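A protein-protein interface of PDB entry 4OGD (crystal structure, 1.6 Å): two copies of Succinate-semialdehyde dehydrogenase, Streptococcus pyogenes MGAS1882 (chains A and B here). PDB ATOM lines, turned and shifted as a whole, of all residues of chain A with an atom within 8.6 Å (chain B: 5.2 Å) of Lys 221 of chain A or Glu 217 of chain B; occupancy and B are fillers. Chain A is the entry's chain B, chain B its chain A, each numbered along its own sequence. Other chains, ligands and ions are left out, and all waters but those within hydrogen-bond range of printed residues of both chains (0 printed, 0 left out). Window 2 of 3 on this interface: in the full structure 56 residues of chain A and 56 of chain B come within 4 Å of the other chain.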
ATOM      1  N   SER A 192      15.001 -21.783   0.843  1.00  0.00           N
ATOM      2  CA  SER A 192      13.654 -22.313   1.060  1.00  0.00           C
ATOM      3  C   SER A 192      13.325 -22.466   2.543  1.00  0.00           C
ATOM      4  O   SER A 192      12.170 -22.253   2.943  1.00  0.00           O
ATOM      5  CB  SER A 192      13.476 -23.644   0.331  1.00  0.00           C
ATOM      6  OG  SER A 192      13.445 -23.439  -1.069  1.00  0.00           O
ATOM      7  N   ILE A 195      12.381 -18.983   3.795  1.00  0.00           N
ATOM      8  CA  ILE A 195      11.034 -18.611   3.365  1.00  0.00           C
ATOM      9  C   ILE A 195       9.957 -19.325   4.187  1.00  0.00           C
ATOM     10  O   ILE A 195       8.908 -18.744   4.495  1.00  0.00           O
ATOM     11  CB  ILE A 195      10.860 -18.868   1.864  1.00  0.00           C
ATOM     12  CG1 ILE A 195      11.821 -17.972   1.081  1.00  0.00           C
ATOM     13  CG2 ILE A 195       9.411 -18.616   1.433  1.00  0.00           C
ATOM     14  CD1 ILE A 195      11.854 -18.227  -0.419  1.00  0.00           C
ATOM     15  N   ALA A 196      10.225 -20.570   4.580  1.00  0.00           N
ATOM     16  CA  ALA A 196       9.264 -21.335   5.380  1.00  0.00           C
ATOM     17  C   ALA A 196       9.302 -21.006   6.870  1.00  0.00           C
ATOM     18  O   ALA A 196       8.443 -21.462   7.632  1.00  0.00           O
ATOM     19  CB  ALA A 196       9.481 -22.846   5.174  1.00  0.00           C
ATOM     20  N   ALA A 213      10.318 -16.677 -10.269  1.00  0.00           N
ATOM     21  CA  ALA A 213       9.272 -17.693 -10.225  1.00  0.00           C
ATOM     22  C   ALA A 213       9.539 -18.749  -9.150  1.00  0.00           C
ATOM     23  O   ALA A 213       8.622 -19.156  -8.441  1.00  0.00           O
ATOM     24  CB  ALA A 213       9.085 -18.347 -11.604  1.00  0.00           C
ATOM     25  N   SER A 214      10.792 -19.190  -9.034  1.00  0.00           N
ATOM     26  CA  SER A 214      11.168 -20.172  -8.014  1.00  0.00           C
ATOM     27  C   SER A 214      10.880 -19.667  -6.607  1.00  0.00           C
ATOM     28  O   SER A 214      10.286 -20.375  -5.776  1.00  0.00           O
ATOM     29  CB  SER A 214      12.660 -20.513  -8.120  1.00  0.00           C
ATOM     30  OG  SER A 214      12.947 -21.198  -9.326  1.00  0.00           O
ATOM     31  N   ILE A 215      11.307 -18.438  -6.351  1.00  0.00           N
ATOM     32  CA  ILE A 215      11.163 -17.812  -5.047  1.00  0.00           C
ATOM     33  C   ILE A 215       9.691 -17.497  -4.731  1.00  0.00           C
ATOM     34  O   ILE A 215       9.212 -17.757  -3.624  1.00  0.00           O
ATOM     35  CB  ILE A 215      12.039 -16.547  -4.966  1.00  0.00           C
ATOM     36  CG1 ILE A 215      13.524 -16.932  -4.964  1.00  0.00           C
ATOM     37  CG2 ILE A 215      11.690 -15.720  -3.743  1.00  0.00           C
ATOM     38  CD1 ILE A 215      13.957 -17.650  -3.723  1.00  0.00           C
ATOM     39  N   ALA A 216       8.966 -16.962  -5.710  1.00  0.00           N
ATOM     40  CA  ALA A 216       7.557 -16.630  -5.498  1.00  0.00           C
ATOM     41  C   ALA A 216       6.718 -17.880  -5.286  1.00  0.00           C
ATOM     42  O   ALA A 216       5.775 -17.867  -4.493  1.00  0.00           O
ATOM     43  CB  ALA A 216       7.002 -15.791  -6.655  1.00  0.00           C
ATOM     44  N   GLU A 217       7.058 -18.963  -5.985  1.00  0.00           N
ATOM     45  CA  GLU A 217       6.354 -20.231  -5.777  1.00  0.00           C
ATOM     46  C   GLU A 217       6.557 -20.706  -4.333  1.00  0.00           C
ATOM     47  O   GLU A 217       5.602 -21.101  -3.654  1.00  0.00           O
ATOM     48  CB  GLU A 217       6.812 -21.304  -6.790  1.00  0.00           C
ATOM     49  CG  GLU A 217       6.065 -22.628  -6.639  1.00  0.00           C
ATOM     50  CD  GLU A 217       6.465 -23.687  -7.660  1.00  0.00           C
ATOM     51  OE1 GLU A 217       7.299 -23.398  -8.541  1.00  0.00           O
ATOM     52  OE2 GLU A 217       5.927 -24.813  -7.578  1.00  0.00           O
ATOM     53  N   GLU A 218       7.798 -20.658  -3.856  1.00  0.00           N
ATOM     54  CA  GLU A 218       8.088 -21.091  -2.489  1.00  0.00           C
ATOM     55  C   GLU A 218       7.423 -20.163  -1.463  1.00  0.00           C
ATOM     56  O   GLU A 218       6.866 -20.626  -0.461  1.00  0.00           O
ATOM     57  CB  GLU A 218       9.606 -21.207  -2.264  1.00  0.00           C
ATOM     58  CG  GLU A 218       9.994 -21.898  -0.957  1.00  0.00           C
ATOM     59  CD  GLU A 218       9.511 -23.346  -0.855  1.00  0.00           C
ATOM     60  OE1 GLU A 218       9.520 -24.063  -1.875  1.00  0.00           O
ATOM     61  OE2 GLU A 218       9.118 -23.767   0.257  1.00  0.00           O
ATOM     62  N   ALA A 219       7.461 -18.858  -1.719  1.00  0.00           N
ATOM     63  CA  ALA A 219       6.781 -17.917  -0.845  1.00  0.00           C
ATOM     64  C   ALA A 219       5.284 -18.193  -0.792  1.00  0.00           C
ATOM     65  O   ALA A 219       4.683 -18.177   0.284  1.00  0.00           O
ATOM     66  CB  ALA A 219       7.049 -16.487  -1.289  1.00  0.00           C
ATOM     67  N   GLY A 220       4.672 -18.433  -1.949  1.00  0.00           N
ATOM     68  CA  GLY A 220       3.239 -18.680  -1.995  1.00  0.00           C
ATOM     69  C   GLY A 220       2.810 -19.877  -1.174  1.00  0.00           C
ATOM     70  O   GLY A 220       1.813 -19.825  -0.456  1.00  0.00           O
ATOM     71  N   LYS A 221       3.571 -20.960  -1.300  1.00  0.00           N
ATOM     72  CA  LYS A 221       3.345 -22.199  -0.568  1.00  0.00           C
ATOM     73  C   LYS A 221       3.352 -21.955   0.932  1.00  0.00           C
ATOM     74  O   LYS A 221       2.686 -22.662   1.696  1.00  0.00           O
ATOM     75  CB  LYS A 221       4.466 -23.180  -0.924  1.00  0.00           C
ATOM     76  CG  LYS A 221       4.444 -24.516  -0.208  1.00  0.00           C
ATOM     77  CD  LYS A 221       5.510 -25.448  -0.807  1.00  0.00           C
ATOM     78  CE  LYS A 221       6.025 -24.900  -2.141  1.00  0.00           C
ATOM     79  NZ  LYS A 221       6.627 -25.928  -3.038  1.00  0.00           N
ATOM     80  N   ASN A 222       4.120 -20.949   1.345  1.00  0.00           N
ATOM     81  CA  ASN A 222       4.277 -20.625   2.751  1.00  0.00           C
ATOM     82  C   ASN A 222       3.522 -19.385   3.201  1.00  0.00           C
ATOM     83  O   ASN A 222       3.742 -18.898   4.318  1.00  0.00           O
ATOM     84  CB  ASN A 222       5.759 -20.489   3.079  1.00  0.00           C
ATOM     85  CG  ASN A 222       6.465 -21.823   3.051  1.00  0.00           C
ATOM     86  OD1 ASN A 222       6.246 -22.661   3.928  1.00  0.00           O
ATOM     87  ND2 ASN A 222       7.288 -22.046   2.024  1.00  0.00           N
ATOM     88  N   LEU A 223       2.639 -18.901   2.329  1.00  0.00           N
ATOM     89  CA  LEU A 223       1.775 -17.744   2.600  1.00  0.00           C
ATOM     90  C   LEU A 223       2.538 -16.450   2.865  1.00  0.00           C
ATOM     91  O   LEU A 223       2.058 -15.581   3.590  1.00  0.00           O
ATOM     92  CB  LEU A 223       0.818 -18.030   3.766  1.00  0.00           C
ATOM     93  CG  LEU A 223      -0.067 -19.268   3.624  1.00  0.00           C
ATOM     94  CD1 LEU A 223      -0.893 -19.472   4.882  1.00  0.00           C
ATOM     95  CD2 LEU A 223      -0.958 -19.140   2.404  1.00  0.00           C
ATOM     96  N   LYS A 224       3.702 -16.303   2.245  1.00  0.00           N
ATOM     97  CA  LYS A 224       4.524 -15.122   2.478  1.00  0.00           C
ATOM     98  C   LYS A 224       4.333 -14.110   1.351  1.00  0.00           C
ATOM     99  O   LYS A 224       4.411 -14.452   0.176  1.00  0.00           O
ATOM    100  CB  LYS A 224       6.004 -15.506   2.581  1.00  0.00           C
ATOM    101  CG  LYS A 224       6.341 -16.501   3.697  1.00  0.00           C
ATOM    102  CD  LYS A 224       5.936 -15.952   5.068  1.00  0.00           C
ATOM    103  CE  LYS A 224       5.943 -17.053   6.137  1.00  0.00           C
ATOM    104  NZ  LYS A 224       7.315 -17.537   6.442  1.00  0.00           N
ATOM    105  N   THR A 226       5.026 -11.223  -1.330  1.00  0.00           N
ATOM    106  CA  THR A 226       6.196 -10.923  -2.156  1.00  0.00           C
ATOM    107  C   THR A 226       6.078  -9.635  -2.939  1.00  0.00           C
ATOM    108  O   THR A 226       4.981  -9.121  -3.177  1.00  0.00           O
ATOM    109  CB  THR A 226       6.466 -11.999  -3.216  1.00  0.00           C
ATOM    110  OG1 THR A 226       5.276 -12.237  -3.982  1.00  0.00           O
ATOM    111  CG2 THR A 226       6.896 -13.281  -2.561  1.00  0.00           C
ATOM    112  N   GLY B 212      -5.502 -21.036   0.121  1.00  0.00           N
ATOM    113  CA  GLY B 212      -4.626 -19.902  -0.101  1.00  0.00           C
ATOM    114  C   GLY B 212      -3.225 -20.321  -0.495  1.00  0.00           C
ATOM    115  O   GLY B 212      -2.653 -19.774  -1.432  1.00  0.00           O
ATOM    116  N   ALA B 213      -2.659 -21.286   0.224  1.00  0.00           N
ATOM    117  CA  ALA B 213      -1.310 -21.734  -0.091  1.00  0.00           C
ATOM    118  C   ALA B 213      -1.241 -22.390  -1.465  1.00  0.00           C
ATOM    119  O   ALA B 213      -0.295 -22.167  -2.216  1.00  0.00           O
ATOM    120  CB  ALA B 213      -0.794 -22.676   0.988  1.00  0.00           C
ATOM    121  N   SER B 214      -2.249 -23.196  -1.793  1.00  0.00           N
ATOM    122  CA  SER B 214      -2.296 -23.861  -3.093  1.00  0.00           C
ATOM    123  C   SER B 214      -2.337 -22.852  -4.240  1.00  0.00           C
ATOM    124  O   SER B 214      -1.586 -22.950  -5.212  1.00  0.00           O
ATOM    125  CB  SER B 214      -3.509 -24.790  -3.157  1.00  0.00           C
ATOM    126  OG  SER B 214      -3.728 -25.261  -4.473  1.00  0.00           O
ATOM    127  N   ILE B 215      -3.213 -21.869  -4.104  1.00  0.00           N
ATOM    128  CA  ILE B 215      -3.396 -20.863  -5.133  1.00  0.00           C
ATOM    129  C   ILE B 215      -2.180 -19.926  -5.220  1.00  0.00           C
ATOM    130  O   ILE B 215      -1.719 -19.594  -6.312  1.00  0.00           O
ATOM    131  CB  ILE B 215      -4.712 -20.086  -4.867  1.00  0.00           C
ATOM    132  CG1 ILE B 215      -5.918 -20.994  -5.130  1.00  0.00           C
ATOM    133  CG2 ILE B 215      -4.797 -18.852  -5.722  1.00  0.00           C
ATOM    134  CD1 ILE B 215      -6.043 -21.426  -6.574  1.00  0.00           C
ATOM    135  N   ALA B 216      -1.635 -19.530  -4.072  1.00  0.00           N
ATOM    136  CA  ALA B 216      -0.507 -18.603  -4.071  1.00  0.00           C
ATOM    137  C   ALA B 216       0.748 -19.268  -4.621  1.00  0.00           C
ATOM    138  O   ALA B 216       1.578 -18.620  -5.274  1.00  0.00           O
ATOM    139  CB  ALA B 216      -0.262 -18.044  -2.667  1.00  0.00           C
ATOM    140  N   GLU B 217       0.898 -20.562  -4.351  1.00  0.00           N
ATOM    141  CA  GLU B 217       2.015 -21.321  -4.911  1.00  0.00           C
ATOM    142  C   GLU B 217       1.947 -21.334  -6.440  1.00  0.00           C
ATOM    143  O   GLU B 217       2.953 -21.087  -7.115  1.00  0.00           O
ATOM    144  CB  GLU B 217       2.029 -22.749  -4.346  1.00  0.00           C
ATOM    145  CG  GLU B 217       3.149 -23.633  -4.878  1.00  0.00           C
ATOM    146  CD  GLU B 217       3.063 -25.063  -4.374  1.00  0.00           C
ATOM    147  OE1 GLU B 217       2.310 -25.315  -3.417  1.00  0.00           O
ATOM    148  OE2 GLU B 217       3.750 -25.933  -4.948  1.00  0.00           O
ATOM    149  N   GLU B 218       0.757 -21.600  -6.984  1.00  0.00           N
ATOM    150  CA  GLU B 218       0.561 -21.640  -8.431  1.00  0.00           C
ATOM    151  C   GLU B 218       0.737 -20.243  -9.045  1.00  0.00           C
ATOM    152  O   GLU B 218       1.322 -20.090 -10.116  1.00  0.00           O
ATOM    153  CB  GLU B 218      -0.822 -22.228  -8.761  1.00  0.00           C
ATOM    154  CG  GLU B 218      -1.102 -22.383 -10.248  1.00  0.00           C
ATOM    155  CD  GLU B 218      -0.239 -23.446 -10.923  1.00  0.00           C
ATOM    156  OE1 GLU B 218       0.148 -24.430 -10.251  1.00  0.00           O
ATOM    157  OE2 GLU B 218       0.044 -23.294 -12.133  1.00  0.00           O
ATOM    158  N   ALA B 219       0.242 -19.220  -8.356  1.00  0.00           N
ATOM    159  CA  ALA B 219       0.421 -17.853  -8.828  1.00  0.00           C
ATOM    160  C   ALA B 219       1.896 -17.467  -8.882  1.00  0.00           C
ATOM    161  O   ALA B 219       2.345 -16.855  -9.846  1.00  0.00           O
ATOM    162  CB  ALA B 219      -0.350 -16.880  -7.952  1.00  0.00           C
ATOM    163  N   GLY B 220       2.652 -17.823  -7.847  1.00  0.00           N
ATOM    164  CA  GLY B 220       4.068 -17.493  -7.814  1.00  0.00           C
ATOM    165  C   GLY B 220       4.819 -18.159  -8.950  1.00  0.00           C
ATOM    166  O   GLY B 220       5.655 -17.528  -9.601  1.00  0.00           O
ATOM    167  N   LYS B 221       4.508 -19.430  -9.195  1.00  0.00           N
ATOM    168  CA  LYS B 221       5.109 -20.177 -10.306  1.00  0.00           C
ATOM    169  C   LYS B 221       4.952 -19.415 -11.625  1.00  0.00           C
ATOM    170  O   LYS B 221       5.822 -19.469 -12.502  1.00  0.00           O
ATOM    171  CB  LYS B 221       4.454 -21.560 -10.405  1.00  0.00           C
ATOM    172  CG  LYS B 221       4.996 -22.478 -11.492  1.00  0.00           C
ATOM    173  CD  LYS B 221       4.295 -23.832 -11.418  1.00  0.00           C
ATOM    174  CE  LYS B 221       4.696 -24.749 -12.566  1.00  0.00           C
ATOM    175  NZ  LYS B 221       4.234 -26.151 -12.323  1.00  0.00           N
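Ala 213 of chain A touches Gly 220 of chain B, and with the chains exchanged Gly 220 of chain A touches Ala 213 of chain B. Ala 213 of chain A touches Lys 221 of chain B, and with the chains exchanged Lys 221 of chain A touches Ala 213 of chain B. Ala 216 of chain A touches Gly 220 of chain B, and with the chains exchanged Gly 220 of chain A touches Ala 216 of chain B. Glu 217 of chain A touches Gly 220 of chain B, and with the chains exchanged Gly 220 of chain A touches Glu 217 of chain B.
Among the printed residues, pairs that only touch across the chains: Ala 213 of chain A with Gly 220 of chain B (3.6 Å), Ala 213 of chain A with Lys 221 of chain B (3.6 Å), Ala 216 of chain A with Gly 220 of chain B (3.6 Å), Glu 217 of chain A with Glu 217 of chain B (3.5 Å), Glu 217 of chain A with Gly 220 of chain B (3.8 Å), Glu 217 of chain A with Lys 221 of chain B (3.8 Å), Gly 220 of chain A with Ala 213 of chain B (3.6 Å), Gly 220 of chain A with Ala 216 of chain B (3.5 Å), Gly 220 of chain A with Glu 217 of chain B (3.8 Å), Lys 221 of chain A with Ala 213 of chain B (3.6 Å), Leu 223 of chain A with Gly 212 of chain B (3.9 Å) and Leu 223 of chain A with Ala 213 of chain B (3.5 Å).
The side-chain carboxylate (OE1) of Glu 218 of chain A is in salt-bridge range of the side-chain amino group (NZ) of Lys 221 of chain A, 3.6 Å away.
Of the 10 printed residues of chain B, 6 touch a printed residue of chain A. Hydrophobic or aromatic side chains of chain B that line the printed part of chain A: Ala 213 and Ala 216. Among the printed residues, 13 pairs touch across the chains.
Of chain B, only Ala 213 (3.6 Å) and Glu 217 (3.5 Å) come within 4 Å of Lys 221 of chain A. Glu 217 of chain B touches just these residues of chain A: Glu 217 (3.5 Å), Gly 220 (3.8 Å) and Lys 221 (3.5 Å). Of chain A, only Gly 220 (3.5 Å) comes within 4 Å of Ala 216 of chain B. Of the printed residues of chain B, Leu 223 of chain A touches Gly 212 and Ala 213. Of the printed residues of chain A, Lys 221 of chain B touches Ala 213 (3.6 Å) and Glu 217 (3.8 Å). Printed residues of chain A within 4 Å of Ala 213 of chain B: Gly 220 (3.6 Å), Lys 221 (3.6 Å) and Leu 223 (3.5 Å). Ser 214 of chain B touches none of the printed residues of chain A. Ile 215 of chain B touches none of the printed residues of chain A. The nearest printed residue of chain A that does not touch Lys 221 of chain B is Ala 216 of chain A (4.8 Å).
The side-chain carboxylate (OE2) of Glu 217 of chain B is in salt-bridge range of the side-chain amino group (NZ) of Lys 221 of chain A (3.5 Å).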
